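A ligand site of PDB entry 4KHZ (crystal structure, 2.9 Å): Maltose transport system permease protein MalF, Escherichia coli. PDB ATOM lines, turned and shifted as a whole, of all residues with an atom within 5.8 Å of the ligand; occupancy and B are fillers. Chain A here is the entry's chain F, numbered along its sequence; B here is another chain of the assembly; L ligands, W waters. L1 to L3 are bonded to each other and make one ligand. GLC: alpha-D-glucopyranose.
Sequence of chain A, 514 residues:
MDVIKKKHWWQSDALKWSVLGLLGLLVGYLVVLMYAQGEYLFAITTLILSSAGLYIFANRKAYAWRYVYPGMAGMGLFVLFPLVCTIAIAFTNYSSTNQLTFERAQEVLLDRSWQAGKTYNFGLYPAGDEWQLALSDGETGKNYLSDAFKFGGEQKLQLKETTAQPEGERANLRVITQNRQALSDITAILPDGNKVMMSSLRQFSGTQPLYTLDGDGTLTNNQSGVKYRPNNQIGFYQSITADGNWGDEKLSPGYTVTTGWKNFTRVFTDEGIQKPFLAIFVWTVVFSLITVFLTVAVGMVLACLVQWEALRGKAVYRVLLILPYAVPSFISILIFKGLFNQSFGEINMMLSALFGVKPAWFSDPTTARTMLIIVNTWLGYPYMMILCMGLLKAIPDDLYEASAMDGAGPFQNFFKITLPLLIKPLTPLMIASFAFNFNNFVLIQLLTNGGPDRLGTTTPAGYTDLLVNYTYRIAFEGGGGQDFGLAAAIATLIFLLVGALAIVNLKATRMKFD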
ATOM      1  N   THR A 291      16.234  29.066  36.325  1.00  0.00           N
ATOM      2  CA  THR A 291      15.473  28.773  35.110  1.00  0.00           C
ATOM      3  C   THR A 291      14.048  28.322  35.440  1.00  0.00           C
ATOM      4  O   THR A 291      13.089  28.842  34.878  1.00  0.00           O
ATOM      5  CB  THR A 291      16.160  27.682  34.260  1.00  0.00           C
ATOM      6  OG1 THR A 291      17.404  28.176  33.752  1.00  0.00           O
ATOM      7  CG2 THR A 291      15.276  27.259  33.093  1.00  0.00           C
ATOM      8  N   THR A 295      10.751  30.562  34.445  1.00  0.00           N
ATOM      9  CA  THR A 295       9.892  29.923  33.436  1.00  0.00           C
ATOM     10  C   THR A 295       8.489  29.668  33.975  1.00  0.00           C
ATOM     11  O   THR A 295       7.496  29.873  33.264  1.00  0.00           O
ATOM     12  CB  THR A 295      10.498  28.597  32.938  1.00  0.00           C
ATOM     13  OG1 THR A 295      10.838  27.764  34.050  1.00  0.00           O
ATOM     14  CG2 THR A 295      11.741  28.855  32.100  1.00  0.00           C
ATOM     15  N   TYR A 325       8.224  28.515  20.941  1.00  0.00           N
ATOM     16  CA  TYR A 325       8.276  27.059  21.090  1.00  0.00           C
ATOM     17  C   TYR A 325       8.158  26.352  19.734  1.00  0.00           C
ATOM     18  O   TYR A 325       8.623  25.228  19.579  1.00  0.00           O
ATOM     19  CB  TYR A 325       7.175  26.582  22.046  1.00  0.00           C
ATOM     20  CG  TYR A 325       7.537  25.376  22.905  1.00  0.00           C
ATOM     21  CD1 TYR A 325       8.736  25.333  23.631  1.00  0.00           C
ATOM     22  CD2 TYR A 325       6.666  24.295  23.032  1.00  0.00           C
ATOM     23  CE1 TYR A 325       9.056  24.253  24.424  1.00  0.00           C
ATOM     24  CE2 TYR A 325       6.983  23.205  23.829  1.00  0.00           C
ATOM     25  CZ  TYR A 325       8.183  23.180  24.517  1.00  0.00           C
ATOM     26  OH  TYR A 325       8.503  22.099  25.310  1.00  0.00           O
ATOM     27  N   SER A 329      14.898  24.717  19.442  1.00  0.00           N
ATOM     28  CA  SER A 329      15.848  25.317  20.393  1.00  0.00           C
ATOM     29  C   SER A 329      17.182  25.641  19.745  1.00  0.00           C
ATOM     30  O   SER A 329      17.701  26.753  19.896  1.00  0.00           O
ATOM     31  CB  SER A 329      16.089  24.388  21.595  1.00  0.00           C
ATOM     32  OG  SER A 329      14.881  23.864  22.116  1.00  0.00           O
ATOM     33  N   ASN A 376      17.526  31.139  28.068  1.00  0.00           N
ATOM     34  CA  ASN A 376      16.868  29.896  28.496  1.00  0.00           C
ATOM     35  C   ASN A 376      15.409  30.130  28.914  1.00  0.00           C
ATOM     36  O   ASN A 376      14.545  29.304  28.622  1.00  0.00           O
ATOM     37  CB  ASN A 376      17.659  29.240  29.626  1.00  0.00           C
ATOM     38  CG  ASN A 376      17.308  27.770  29.819  1.00  0.00           C
ATOM     39  OD1 ASN A 376      17.563  27.215  30.882  1.00  0.00           O
ATOM     40  ND2 ASN A 376      16.758  27.142  28.784  1.00  0.00           N
ATOM     41  N   LEU A 379      13.208  30.312  25.907  1.00  0.00           N
ATOM     42  CA  LEU A 379      12.898  28.986  25.392  1.00  0.00           C
ATOM     43  C   LEU A 379      11.948  28.207  26.302  1.00  0.00           C
ATOM     44  O   LEU A 379      11.129  27.418  25.825  1.00  0.00           O
ATOM     45  CB  LEU A 379      14.185  28.163  25.225  1.00  0.00           C
ATOM     46  CG  LEU A 379      15.165  28.503  24.098  1.00  0.00           C
ATOM     47  CD1 LEU A 379      16.088  29.648  24.498  1.00  0.00           C
ATOM     48  CD2 LEU A 379      15.979  27.278  23.737  1.00  0.00           C
ATOM     49  N   GLY A 380      12.054  28.438  27.602  1.00  0.00           N
ATOM     50  CA  GLY A 380      11.397  27.598  28.618  1.00  0.00           C
ATOM     51  C   GLY A 380       9.976  27.971  29.015  1.00  0.00           C
ATOM     52  O   GLY A 380       9.201  27.095  29.385  1.00  0.00           O
ATOM     53  N   TYR A 381       9.641  29.266  28.942  1.00  0.00           N
ATOM     54  CA  TYR A 381       8.343  29.740  29.403  1.00  0.00           C
ATOM     55  C   TYR A 381       7.147  29.179  28.636  1.00  0.00           C
ATOM     56  O   TYR A 381       6.099  28.931  29.229  1.00  0.00           O
ATOM     57  CB  TYR A 381       8.287  31.290  29.453  1.00  0.00           C
ATOM     58  CG  TYR A 381       7.943  31.989  28.151  1.00  0.00           C
ATOM     59  CD1 TYR A 381       6.616  32.106  27.729  1.00  0.00           C
ATOM     60  CD2 TYR A 381       8.936  32.568  27.373  1.00  0.00           C
ATOM     61  CE1 TYR A 381       6.302  32.755  26.544  1.00  0.00           C
ATOM     62  CE2 TYR A 381       8.625  33.225  26.184  1.00  0.00           C
ATOM     63  CZ  TYR A 381       7.309  33.310  25.776  1.00  0.00           C
ATOM     64  OH  TYR A 381       6.985  33.947  24.607  1.00  0.00           O
ATOM     65  N   TYR A 383       6.705  26.156  27.409  1.00  0.00           N
ATOM     66  CA  TYR A 383       6.429  24.839  27.987  1.00  0.00           C
ATOM     67  C   TYR A 383       5.640  24.973  29.281  1.00  0.00           C
ATOM     68  O   TYR A 383       4.683  24.240  29.509  1.00  0.00           O
ATOM     69  CB  TYR A 383       7.722  24.065  28.226  1.00  0.00           C
ATOM     70  CG  TYR A 383       7.533  22.801  29.039  1.00  0.00           C
ATOM     71  CD1 TYR A 383       6.716  21.774  28.578  1.00  0.00           C
ATOM     72  CD2 TYR A 383       8.165  22.632  30.258  1.00  0.00           C
ATOM     73  CE1 TYR A 383       6.531  20.616  29.322  1.00  0.00           C
ATOM     74  CE2 TYR A 383       7.992  21.482  31.003  1.00  0.00           C
ATOM     75  CZ  TYR A 383       7.173  20.472  30.529  1.00  0.00           C
ATOM     76  OH  TYR A 383       7.012  19.331  31.276  1.00  0.00           O
ATOM     77  N   MET A 384       6.050  25.917  30.132  1.00  0.00           N
ATOM     78  CA  MET A 384       5.379  26.160  31.403  1.00  0.00           C
ATOM     79  C   MET A 384       4.016  26.812  31.222  1.00  0.00           C
ATOM     80  O   MET A 384       3.090  26.522  31.974  1.00  0.00           O
ATOM     81  CB  MET A 384       6.245  27.060  32.305  1.00  0.00           C
ATOM     82  CG  MET A 384       7.469  26.368  32.887  1.00  0.00           C
ATOM     83  SD  MET A 384       7.062  25.151  34.146  1.00  0.00           S
ATOM     84  CE  MET A 384       7.325  23.629  33.252  1.00  0.00           C
ATOM     85  N   LEU A 429       6.247  18.281  37.809  1.00  0.00           N
ATOM     86  CA  LEU A 429       6.690  18.751  36.505  1.00  0.00           C
ATOM     87  C   LEU A 429       7.865  19.715  36.594  1.00  0.00           C
ATOM     88  O   LEU A 429       8.731  19.725  35.721  1.00  0.00           O
ATOM     89  CB  LEU A 429       5.526  19.406  35.742  1.00  0.00           C
ATOM     90  CG  LEU A 429       4.418  18.425  35.345  1.00  0.00           C
ATOM     91  CD1 LEU A 429       3.093  19.121  35.089  1.00  0.00           C
ATOM     92  CD2 LEU A 429       4.841  17.594  34.138  1.00  0.00           C
ATOM     93  N   ALA A 432      10.945  17.885  37.566  1.00  0.00           N
ATOM     94  CA  ALA A 432      11.351  17.257  36.306  1.00  0.00           C
ATOM     95  C   ALA A 432      11.960  18.288  35.360  1.00  0.00           C
ATOM     96  O   ALA A 432      12.865  17.967  34.585  1.00  0.00           O
ATOM     97  CB  ALA A 432      10.165  16.576  35.638  1.00  0.00           C
ATOM     98  N   SER A 433      11.457  19.522  35.421  1.00  0.00           N
ATOM     99  CA  SER A 433      12.047  20.631  34.677  1.00  0.00           C
ATOM    100  C   SER A 433      13.421  21.006  35.216  1.00  0.00           C
ATOM    101  O   SER A 433      14.284  21.469  34.459  1.00  0.00           O
ATOM    102  CB  SER A 433      11.129  21.866  34.726  1.00  0.00           C
ATOM    103  OG  SER A 433      11.596  22.882  33.859  1.00  0.00           O
ATOM    104  N   PHE A 434      13.628  20.826  36.517  1.00  0.00           N
ATOM    105  CA  PHE A 434      14.932  21.062  37.151  1.00  0.00           C
ATOM    106  C   PHE A 434      15.979  20.074  36.636  1.00  0.00           C
ATOM    107  O   PHE A 434      17.092  20.469  36.309  1.00  0.00           O
ATOM    108  CB  PHE A 434      14.821  20.956  38.680  1.00  0.00           C
ATOM    109  CG  PHE A 434      16.155  20.957  39.383  1.00  0.00           C
ATOM    110  CD1 PHE A 434      16.776  19.767  39.737  1.00  0.00           C
ATOM    111  CD2 PHE A 434      16.798  22.157  39.674  1.00  0.00           C
ATOM    112  CE1 PHE A 434      17.992  19.761  40.382  1.00  0.00           C
ATOM    113  CE2 PHE A 434      18.026  22.159  40.319  1.00  0.00           C
ATOM    114  CZ  PHE A 434      18.626  20.962  40.667  1.00  0.00           C
ATOM    115  N   PHE A 436      15.952  18.428  33.849  1.00  0.00           N
ATOM    116  CA  PHE A 436      16.211  18.704  32.431  1.00  0.00           C
ATOM    117  C   PHE A 436      17.306  19.758  32.298  1.00  0.00           C
ATOM    118  O   PHE A 436      18.320  19.536  31.647  1.00  0.00           O
ATOM    119  CB  PHE A 436      14.932  19.189  31.735  1.00  0.00           C
ATOM    120  CG  PHE A 436      15.124  19.521  30.282  1.00  0.00           C
ATOM    121  CD1 PHE A 436      15.470  20.794  29.890  1.00  0.00           C
ATOM    122  CD2 PHE A 436      14.956  18.548  29.316  1.00  0.00           C
ATOM    123  CE1 PHE A 436      15.649  21.103  28.552  1.00  0.00           C
ATOM    124  CE2 PHE A 436      15.136  18.843  27.974  1.00  0.00           C
ATOM    125  CZ  PHE A 436      15.478  20.121  27.590  1.00  0.00           C
ATOM    126  N   ASN A 437      17.073  20.911  32.928  1.00  0.00           N
ATOM    127  CA  ASN A 437      18.019  22.022  32.875  1.00  0.00           C
ATOM    128  C   ASN A 437      19.347  21.699  33.555  1.00  0.00           C
ATOM    129  O   ASN A 437      20.393  22.221  33.146  1.00  0.00           O
ATOM    130  CB  ASN A 437      17.415  23.275  33.516  1.00  0.00           C
ATOM    131  CG  ASN A 437      16.300  23.865  32.679  1.00  0.00           C
ATOM    132  OD1 ASN A 437      15.159  23.975  33.113  1.00  0.00           O
ATOM    133  ND2 ASN A 437      16.636  24.244  31.443  1.00  0.00           N
ATOM    134  N   ASN A 440      21.216  20.422  30.695  1.00  0.00           N
ATOM    135  CA  ASN A 440      20.901  21.074  29.415  1.00  0.00           C
ATOM    136  C   ASN A 440      22.196  21.296  28.642  1.00  0.00           C
ATOM    137  O   ASN A 440      22.835  22.349  28.740  1.00  0.00           O
ATOM    138  CB  ASN A 440      20.142  22.389  29.641  1.00  0.00           C
ATOM    139  CG  ASN A 440      19.150  22.690  28.536  1.00  0.00           C
ATOM    140  OD1 ASN A 440      18.139  23.366  28.765  1.00  0.00           O
ATOM    141  ND2 ASN A 440      19.413  22.192  27.337  1.00  0.00           N
ATOM    142  N   LEU A 443      22.110  23.770  25.034  1.00  0.00           N
ATOM    143  CA  LEU A 443      22.102  25.224  25.241  1.00  0.00           C
ATOM    144  C   LEU A 443      23.503  25.773  25.452  1.00  0.00           C
ATOM    145  O   LEU A 443      23.883  26.759  24.823  1.00  0.00           O
ATOM    146  CB  LEU A 443      21.213  25.587  26.445  1.00  0.00           C
ATOM    147  CG  LEU A 443      21.155  27.068  26.817  1.00  0.00           C
ATOM    148  CD1 LEU A 443      20.601  27.896  25.672  1.00  0.00           C
ATOM    149  CD2 LEU A 443      20.331  27.272  28.083  1.00  0.00           C
ATOM    150  N   LEU B 172       8.968  10.204  31.862  1.00  0.00           N
ATOM    151  CA  LEU B 172       8.059  11.333  32.093  1.00  0.00           C
ATOM    152  C   LEU B 172       6.703  11.116  31.432  1.00  0.00           C
ATOM    153  O   LEU B 172       5.677  11.512  31.973  1.00  0.00           O
ATOM    154  CB  LEU B 172       8.657  12.643  31.561  1.00  0.00           C
ATOM    155  CG  LEU B 172       9.827  13.243  32.340  1.00  0.00           C
ATOM    156  CD1 LEU B 172      10.322  14.503  31.641  1.00  0.00           C
ATOM    157  CD2 LEU B 172       9.435  13.540  33.777  1.00  0.00           C
ATOM    158  N   LEU B 221       5.046  17.202  22.508  1.00  0.00           N
ATOM    159  CA  LEU B 221       6.246  17.337  23.339  1.00  0.00           C
ATOM    160  C   LEU B 221       7.346  16.376  22.874  1.00  0.00           C
ATOM    161  O   LEU B 221       8.527  16.751  22.860  1.00  0.00           O
ATOM    162  CB  LEU B 221       5.910  17.079  24.809  1.00  0.00           C
ATOM    163  CG  LEU B 221       4.966  18.098  25.451  1.00  0.00           C
ATOM    164  CD1 LEU B 221       4.466  17.590  26.803  1.00  0.00           C
ATOM    165  CD2 LEU B 221       5.639  19.455  25.600  1.00  0.00           C
ATOM    166  N   ILE B 224       8.446  17.863  19.339  1.00  0.00           N
ATOM    167  CA  ILE B 224       9.312  19.024  19.526  1.00  0.00           C
ATOM    168  C   ILE B 224      10.681  18.585  20.042  1.00  0.00           C
ATOM    169  O   ILE B 224      11.717  19.089  19.587  1.00  0.00           O
ATOM    170  CB  ILE B 224       8.668  20.045  20.486  1.00  0.00           C
ATOM    171  CG1 ILE B 224       7.452  20.698  19.829  1.00  0.00           C
ATOM    172  CG2 ILE B 224       9.679  21.122  20.886  1.00  0.00           C
ATOM    173  CD1 ILE B 224       6.499  21.361  20.798  1.00  0.00           C
ATOM    174  N   ALA B 225      10.679  17.650  20.985  1.00  0.00           N
ATOM    175  CA  ALA B 225      11.914  17.100  21.531  1.00  0.00           C
ATOM    176  C   ALA B 225      12.802  16.532  20.411  1.00  0.00           C
ATOM    177  O   ALA B 225      13.991  16.825  20.352  1.00  0.00           O
ATOM    178  CB  ALA B 225      11.620  16.028  22.568  1.00  0.00           C
ATOM    179  N   THR B 228      14.322  19.186  17.862  1.00  0.00           N
ATOM    180  CA  THR B 228      15.432  19.977  18.402  1.00  0.00           C
ATOM    181  C   THR B 228      16.632  19.150  18.902  1.00  0.00           C
ATOM    182  O   THR B 228      17.645  19.719  19.315  1.00  0.00           O
ATOM    183  CB  THR B 228      14.962  20.928  19.529  1.00  0.00           C
ATOM    184  OG1 THR B 228      15.982  21.893  19.797  1.00  0.00           O
ATOM    185  CG2 THR B 228      14.638  20.161  20.820  1.00  0.00           C
HETATM  186  O4  GLC L   1      11.247  17.808  29.153  1.00  0.00           O
HETATM  187  C1  GLC L   2      10.213  18.808  29.007  1.00  0.00           C
HETATM  188  C2  GLC L   2      10.021  19.159  27.534  1.00  0.00           C
HETATM  189  C3  GLC L   2      11.148  20.029  26.987  1.00  0.00           C
HETATM  190  C4  GLC L   2      11.310  21.240  27.883  1.00  0.00           C
HETATM  191  C5  GLC L   2      11.549  20.798  29.324  1.00  0.00           C
HETATM  192  C6  GLC L   2      11.667  22.009  30.236  1.00  0.00           C
HETATM  193  O2  GLC L   2       9.915  17.989  26.745  1.00  0.00           O
HETATM  194  O3  GLC L   2      10.828  20.460  25.681  1.00  0.00           O
HETATM  195  O4  GLC L   2      12.368  22.061  27.425  1.00  0.00           O
HETATM  196  O5  GLC L   2      10.492  19.963  29.779  1.00  0.00           O
HETATM  197  O6  GLC L   2      11.228  21.687  31.536  1.00  0.00           O
HETATM  198  C1  GLC L   3      11.967  23.412  27.120  1.00  0.00           C
HETATM  199  C2  GLC L   3      12.543  23.840  25.783  1.00  0.00           C
HETATM  200  C3  GLC L   3      14.043  24.066  25.857  1.00  0.00           C
HETATM  201  C4  GLC L   3      14.438  24.916  27.068  1.00  0.00           C
HETATM  202  C5  GLC L   3      13.734  24.446  28.337  1.00  0.00           C
HETATM  203  C6  GLC L   3      13.990  25.414  29.487  1.00  0.00           C
HETATM  204  O2  GLC L   3      12.276  22.837  24.822  1.00  0.00           O
HETATM  205  O3  GLC L   3      14.464  24.707  24.676  1.00  0.00           O
HETATM  206  O4  GLC L   3      15.841  24.876  27.241  1.00  0.00           O
HETATM  207  O5  GLC L   3      12.349  24.340  28.113  1.00  0.00           O
HETATM  208  O6  GLC L   3      13.172  25.079  30.578  1.00  0.00           O
HETATM  209  O   HOH W   1      17.277  23.185  24.994  1.00  0.00           O
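The side-chain amide oxygen (OD1) of Asn 376 sits at hydrogen-bond distance from the side-chain hydroxyl (OG1) of Thr 291, 3.0 Å away.
The backbone carbonyl oxygen (O) of Ser 433 sits close to the side-chain amide oxygen (OD1) of Asn 437 (3.0 Å).
The backbone NH of Ser 329 sits at hydrogen-bond distance from the side-chain hydroxyl of Thr 228 of chain B.
OD1 of Asn 376 lies within hydrogen-bond range of ND2 of Asn 437 (3.2 Å).
The backbone carbonyl oxygen of Thr 291 is in hydrogen-bond range of the side-chain hydroxyl of Thr 295 (2.6 Å).
The side-chain amide nitrogen (ND2) of Asn 437 sits at hydrogen-bond distance from the side-chain amide oxygen (OD1) of Asn 440.
The side-chain amide oxygen of Asn 437 is in hydrogen-bond range of an oxygen (O6) of GLC L3, 3.4 Å away.
The side-chain hydroxyl (OG) of Ser 433 sits at hydrogen-bond distance from an oxygen (O6) of GLC L2, at 2.6 Å.
OD1 of Asn 440 sits at hydrogen-bond distance from O4 of GLC L3, at 3.1 Å.
The side-chain hydroxyl (OH) of Tyr 325 sits at hydrogen-bond distance from an oxygen (O3) of GLC L2 (2.9 Å).
ND2 of Asn 376 is in hydrogen-bond range of O4 of GLC L3, 2.9 Å away.
An oxygen (O3) of GLC L3 lies within hydrogen-bond range of the side-chain hydroxyl (OG) of Ser 329, 2.7 Å away.
Residues that only touch the ligand: Leu 379 (3.1 Å), Tyr 383 (3.2 Å), Gly 380 (3.4 Å), Phe 436 (3.6 Å) and Thr 291 (3.9 Å).
Hydrophobic or aromatic side chains that line the ligand: Tyr 325, Leu 379, Tyr 383 and Phe 436.
The nearest printed residue that does not touch the ligand is Leu 172 of chain B (4.2 Å).
Water W1 lies within hydrogen-bond range of O4 of GLC L3 (3.2 Å) and ND2 of Asn 440 (3.3 Å).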
